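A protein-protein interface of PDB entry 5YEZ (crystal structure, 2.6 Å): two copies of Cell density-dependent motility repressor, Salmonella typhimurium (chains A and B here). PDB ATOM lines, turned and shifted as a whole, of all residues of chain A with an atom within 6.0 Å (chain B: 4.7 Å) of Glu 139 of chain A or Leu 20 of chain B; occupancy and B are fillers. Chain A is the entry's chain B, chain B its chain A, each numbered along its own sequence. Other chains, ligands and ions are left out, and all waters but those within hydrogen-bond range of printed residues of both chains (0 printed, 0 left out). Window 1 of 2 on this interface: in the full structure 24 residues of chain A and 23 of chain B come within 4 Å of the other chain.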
ATOM      1  N   LEU A  20     -33.721  15.439   7.501  1.00  0.00           N
ATOM      2  CA  LEU A  20     -33.022  14.273   8.033  1.00  0.00           C
ATOM      3  C   LEU A  20     -33.319  14.073   9.514  1.00  0.00           C
ATOM      4  O   LEU A  20     -33.559  12.944   9.956  1.00  0.00           O
ATOM      5  CB  LEU A  20     -31.517  14.408   7.799  1.00  0.00           C
ATOM      6  CG  LEU A  20     -30.654  13.145   7.921  1.00  0.00           C
ATOM      7  CD1 LEU A  20     -30.233  12.876   9.364  1.00  0.00           C
ATOM      8  CD2 LEU A  20     -31.377  11.940   7.339  1.00  0.00           C
ATOM      9  N   MET A 137     -27.254  22.404   2.192  1.00  0.00           N
ATOM     10  CA  MET A 137     -27.330  21.049   2.728  1.00  0.00           C
ATOM     11  C   MET A 137     -26.483  20.983   3.993  1.00  0.00           C
ATOM     12  O   MET A 137     -25.250  21.041   3.929  1.00  0.00           O
ATOM     13  CB  MET A 137     -26.856  20.029   1.697  1.00  0.00           C
ATOM     14  CG  MET A 137     -27.694  19.982   0.435  1.00  0.00           C
ATOM     15  SD  MET A 137     -26.983  18.885  -0.807  1.00  0.00           S
ATOM     16  CE  MET A 137     -25.683  19.921  -1.473  1.00  0.00           C
ATOM     17  N   SER A 138     -27.143  20.862   5.148  1.00  0.00           N
ATOM     18  CA  SER A 138     -26.413  20.832   6.411  1.00  0.00           C
ATOM     19  C   SER A 138     -25.526  19.599   6.522  1.00  0.00           C
ATOM     20  O   SER A 138     -24.493  19.640   7.199  1.00  0.00           O
ATOM     21  CB  SER A 138     -27.387  20.887   7.585  1.00  0.00           C
ATOM     22  OG  SER A 138     -26.694  21.046   8.811  1.00  0.00           O
ATOM     23  N   GLU A 139     -25.908  18.500   5.869  1.00  0.00           N
ATOM     24  CA  GLU A 139     -25.076  17.303   5.901  1.00  0.00           C
ATOM     25  C   GLU A 139     -23.749  17.535   5.188  1.00  0.00           C
ATOM     26  O   GLU A 139     -22.699  17.080   5.655  1.00  0.00           O
ATOM     27  CB  GLU A 139     -25.827  16.126   5.278  1.00  0.00           C
ATOM     28  CG  GLU A 139     -25.175  14.773   5.517  1.00  0.00           C
ATOM     29  CD  GLU A 139     -25.262  14.323   6.965  1.00  0.00           C
ATOM     30  OE1 GLU A 139     -24.493  13.416   7.352  1.00  0.00           O
ATOM     31  OE2 GLU A 139     -26.097  14.873   7.715  1.00  0.00           O
ATOM     32  N   LEU A 140     -23.776  18.249   4.060  1.00  0.00           N
ATOM     33  CA  LEU A 140     -22.539  18.538   3.342  1.00  0.00           C
ATOM     34  C   LEU A 140     -21.639  19.468   4.146  1.00  0.00           C
ATOM     35  O   LEU A 140     -20.421  19.258   4.208  1.00  0.00           O
ATOM     36  CB  LEU A 140     -22.856  19.143   1.975  1.00  0.00           C
ATOM     37  CG  LEU A 140     -21.659  19.446   1.072  1.00  0.00           C
ATOM     38  CD1 LEU A 140     -20.734  18.245   0.994  1.00  0.00           C
ATOM     39  CD2 LEU A 140     -22.130  19.853  -0.315  1.00  0.00           C
ATOM     40  N   LEU A 141     -22.214  20.501   4.766  1.00  0.00           N
ATOM     41  CA  LEU A 141     -21.416  21.391   5.603  1.00  0.00           C
ATOM     42  C   LEU A 141     -20.842  20.656   6.806  1.00  0.00           C
ATOM     43  O   LEU A 141     -19.728  20.960   7.246  1.00  0.00           O
ATOM     44  CB  LEU A 141     -22.257  22.581   6.066  1.00  0.00           C
ATOM     45  CG  LEU A 141     -22.876  23.468   4.986  1.00  0.00           C
ATOM     46  CD1 LEU A 141     -23.630  24.631   5.617  1.00  0.00           C
ATOM     47  CD2 LEU A 141     -21.810  23.977   4.033  1.00  0.00           C
ATOM     48  N   LYS A 142     -21.584  19.688   7.346  1.00  0.00           N
ATOM     49  CA  LYS A 142     -21.109  18.947   8.509  1.00  0.00           C
ATOM     50  C   LYS A 142     -19.876  18.119   8.168  1.00  0.00           C
ATOM     51  O   LYS A 142     -18.886  18.125   8.910  1.00  0.00           O
ATOM     52  CB  LYS A 142     -22.227  18.058   9.050  1.00  0.00           C
ATOM     53  CG  LYS A 142     -21.934  17.445  10.406  1.00  0.00           C
ATOM     54  CD  LYS A 142     -21.994  15.929  10.348  1.00  0.00           C
ATOM     55  CE  LYS A 142     -22.406  15.345  11.687  1.00  0.00           C
ATOM     56  NZ  LYS A 142     -22.562  13.866  11.624  1.00  0.00           N
ATOM     57  N   GLN A 143     -19.916  17.402   7.044  1.00  0.00           N
ATOM     58  CA  GLN A 143     -18.791  16.555   6.667  1.00  0.00           C
ATOM     59  C   GLN A 143     -17.609  17.366   6.149  1.00  0.00           C
ATOM     60  O   GLN A 143     -16.461  16.926   6.275  1.00  0.00           O
ATOM     61  CB  GLN A 143     -19.234  15.529   5.624  1.00  0.00           C
ATOM     62  CG  GLN A 143     -20.495  14.775   6.017  1.00  0.00           C
ATOM     63  CD  GLN A 143     -20.482  13.331   5.559  1.00  0.00           C
ATOM     64  OE1 GLN A 143     -19.613  12.552   5.950  1.00  0.00           O
ATOM     65  NE2 GLN A 143     -21.450  12.966   4.724  1.00  0.00           N
ATOM     66  N   VAL A 144     -17.862  18.541   5.570  1.00  0.00           N
ATOM     67  CA  VAL A 144     -16.764  19.416   5.172  1.00  0.00           C
ATOM     68  C   VAL A 144     -16.081  20.001   6.403  1.00  0.00           C
ATOM     69  O   VAL A 144     -14.855  20.166   6.431  1.00  0.00           O
ATOM     70  CB  VAL A 144     -17.273  20.514   4.219  1.00  0.00           C
ATOM     71  CG1 VAL A 144     -16.241  21.620   4.065  1.00  0.00           C
ATOM     72  CG2 VAL A 144     -17.614  19.920   2.861  1.00  0.00           C
ATOM     73  N   HIS B  16     -27.413  14.747  -5.655  1.00  0.00           N
ATOM     74  CA  HIS B  16     -27.525  14.726  -4.199  1.00  0.00           C
ATOM     75  C   HIS B  16     -26.657  13.634  -3.587  1.00  0.00           C
ATOM     76  O   HIS B  16     -26.014  13.851  -2.553  1.00  0.00           O
ATOM     77  CB  HIS B  16     -28.986  14.543  -3.793  1.00  0.00           C
ATOM     78  CG  HIS B  16     -29.300  15.051  -2.421  1.00  0.00           C
ATOM     79  ND1 HIS B  16     -28.650  14.598  -1.293  1.00  0.00           N
ATOM     80  CD2 HIS B  16     -30.193  15.975  -1.997  1.00  0.00           C
ATOM     81  CE1 HIS B  16     -29.130  15.221  -0.232  1.00  0.00           C
ATOM     82  NE2 HIS B  16     -30.068  16.061  -0.631  1.00  0.00           N
ATOM     83  N   SER B  17     -26.619  12.457  -4.214  1.00  0.00           N
ATOM     84  CA  SER B  17     -25.799  11.371  -3.687  1.00  0.00           C
ATOM     85  C   SER B  17     -24.315  11.662  -3.862  1.00  0.00           C
ATOM     86  O   SER B  17     -23.517  11.422  -2.949  1.00  0.00           O
ATOM     87  CB  SER B  17     -26.171  10.056  -4.371  1.00  0.00           C
ATOM     88  OG  SER B  17     -25.530   8.959  -3.742  1.00  0.00           O
ATOM     89  N   LEU B  18     -23.926  12.184  -5.028  1.00  0.00           N
ATOM     90  CA  LEU B  18     -22.515  12.447  -5.286  1.00  0.00           C
ATOM     91  C   LEU B  18     -22.007  13.646  -4.495  1.00  0.00           C
ATOM     92  O   LEU B  18     -20.838  13.668  -4.093  1.00  0.00           O
ATOM     93  CB  LEU B  18     -22.291  12.668  -6.781  1.00  0.00           C
ATOM     94  CG  LEU B  18     -21.782  11.464  -7.574  1.00  0.00           C
ATOM     95  CD1 LEU B  18     -21.642  11.813  -9.046  1.00  0.00           C
ATOM     96  CD2 LEU B  18     -20.458  10.978  -7.006  1.00  0.00           C
ATOM     97  N   SER B  19     -22.862  14.645  -4.260  1.00  0.00           N
ATOM     98  CA  SER B  19     -22.411  15.855  -3.583  1.00  0.00           C
ATOM     99  C   SER B  19     -22.052  15.592  -2.127  1.00  0.00           C
ATOM    100  O   SER B  19     -21.219  16.306  -1.558  1.00  0.00           O
ATOM    101  CB  SER B  19     -23.485  16.940  -3.670  1.00  0.00           C
ATOM    102  OG  SER B  19     -24.658  16.551  -2.977  1.00  0.00           O
ATOM    103  N   LEU B  20     -22.662  14.582  -1.510  1.00  0.00           N
ATOM    104  CA  LEU B  20     -22.447  14.299  -0.098  1.00  0.00           C
ATOM    105  C   LEU B  20     -21.452  13.172   0.148  1.00  0.00           C
ATOM    106  O   LEU B  20     -21.106  12.919   1.306  1.00  0.00           O
ATOM    107  CB  LEU B  20     -23.778  13.957   0.582  1.00  0.00           C
ATOM    108  CG  LEU B  20     -24.526  15.102   1.271  1.00  0.00           C
ATOM    109  CD1 LEU B  20     -24.643  16.319   0.361  1.00  0.00           C
ATOM    110  CD2 LEU B  20     -25.901  14.643   1.730  1.00  0.00           C
ATOM    111  N   GLY B  21     -20.984  12.499  -0.898  1.00  0.00           N
ATOM    112  CA  GLY B  21     -20.081  11.380  -0.716  1.00  0.00           C
ATOM    113  C   GLY B  21     -18.718  11.577  -1.348  1.00  0.00           C
ATOM    114  O   GLY B  21     -17.736  10.963  -0.920  1.00  0.00           O
ATOM    115  N   LEU B  22     -18.644  12.432  -2.363  1.00  0.00           N
ATOM    116  CA  LEU B  22     -17.408  12.669  -3.098  1.00  0.00           C
ATOM    117  C   LEU B  22     -16.859  14.076  -2.927  1.00  0.00           C
ATOM    118  O   LEU B  22     -15.640  14.251  -2.856  1.00  0.00           O
ATOM    119  CB  LEU B  22     -17.627  12.388  -4.590  1.00  0.00           C
ATOM    120  CG  LEU B  22     -16.554  12.878  -5.562  1.00  0.00           C
ATOM    121  CD1 LEU B  22     -15.317  11.992  -5.500  1.00  0.00           C
ATOM    122  CD2 LEU B  22     -17.112  12.932  -6.972  1.00  0.00           C
ATOM    123  N   PRO B  24     -16.803  16.293  -0.295  1.00  0.00           N
ATOM    124  CA  PRO B  24     -15.931  16.553   0.864  1.00  0.00           C
ATOM    125  C   PRO B  24     -14.517  16.028   0.688  1.00  0.00           C
ATOM    126  O   PRO B  24     -13.566  16.661   1.163  1.00  0.00           O
ATOM    127  CB  PRO B  24     -16.657  15.845   2.015  1.00  0.00           C
ATOM    128  CG  PRO B  24     -18.076  15.827   1.602  1.00  0.00           C
ATOM    129  CD  PRO B  24     -18.061  15.642   0.114  1.00  0.00           C
ATOM    130  N   GLU B 139     -28.809  10.729   1.611  1.00  0.00           N
ATOM    131  CA  GLU B 139     -28.612  10.555   3.045  1.00  0.00           C
ATOM    132  C   GLU B 139     -29.925  10.273   3.761  1.00  0.00           C
ATOM    133  O   GLU B 139     -29.942   9.552   4.766  1.00  0.00           O
ATOM    134  CB  GLU B 139     -27.934  11.792   3.636  1.00  0.00           C
ATOM    135  CG  GLU B 139     -26.479  11.572   4.019  1.00  0.00           C
ATOM    136  CD  GLU B 139     -26.324  10.719   5.263  1.00  0.00           C
ATOM    137  OE1 GLU B 139     -25.804   9.588   5.151  1.00  0.00           O
ATOM    138  OE2 GLU B 139     -26.722  11.180   6.354  1.00  0.00           O
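NE2 of Gln 143 of chain A sits at hydrogen-bond distance from O of Leu 20 of chain B, at 3.4 Å.
The side-chain carboxylate of Glu 139 of chain B sits close to the side-chain carboxylate of Glu 139 of chain A (3.3 Å).
The side-chain hydroxyl of Ser 19 of chain B is in hydrogen-bond range of the backbone carbonyl oxygen of His 16 of chain B (3.1 Å).
Of the 9 printed residues of chain A, 5 touch a printed residue of chain B.
Hydrophobic or aromatic side chains of chain A within 4 Å of the printed part of chain B: Leu 20, Met 137 and Leu 140.
Of the 9 printed residues of chain B, 4 touch a printed residue of chain A.
Among the printed residues, no Asp or Glu carboxylate lies within 4 Å of a Lys or Arg side-chain nitrogen of the other chain.
Leu 20 of chain A touches Glu 139 of chain B, and with the chains exchanged Glu 139 of chain A touches Leu 20 of chain B.
Glu 139 of chain A touches its own counterpart, Glu 139 of chain B.
Positions printed for both chains: 20 and 139.
Glu 139 of chain A touches just these residues of chain B: Leu 20 (3.8 Å) and Glu 139 (3.3 Å).
Of the printed residues of chain B, Leu 140 of chain A touches Ser 19, Leu 20 and Pro 24.
Of the printed residues of chain A, Ser 19 of chain B touches Met 137 and Leu 140.
The nearest printed residue of chain B that does not touch Leu 20 of chain A is Leu 20 of chain B (7.9 Å).
O of Glu 139 of chain B touches CD2 of Leu 20 of chain A, 3.8 Å away.
Met 137 of chain A touches Ser 19 of chain B (CE to OG, 3.8 Å).
Met 137 of chain A touches Leu 20 of chain B (SD to CD1, 3.7 Å).
CB of Glu 139 of chain A touches CD2 of Leu 20 of chain B, at 3.8 Å.
Leu 140 of chain A touches Ser 19 of chain B (CD1 to O, 3.2 Å).
Leu 140 of chain A touches Leu 20 of chain B (CB to CD1, 3.7 Å).
Leu 140 of chain A touches Pro 24 of chain B (CD1 to CG, 3.6 Å).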
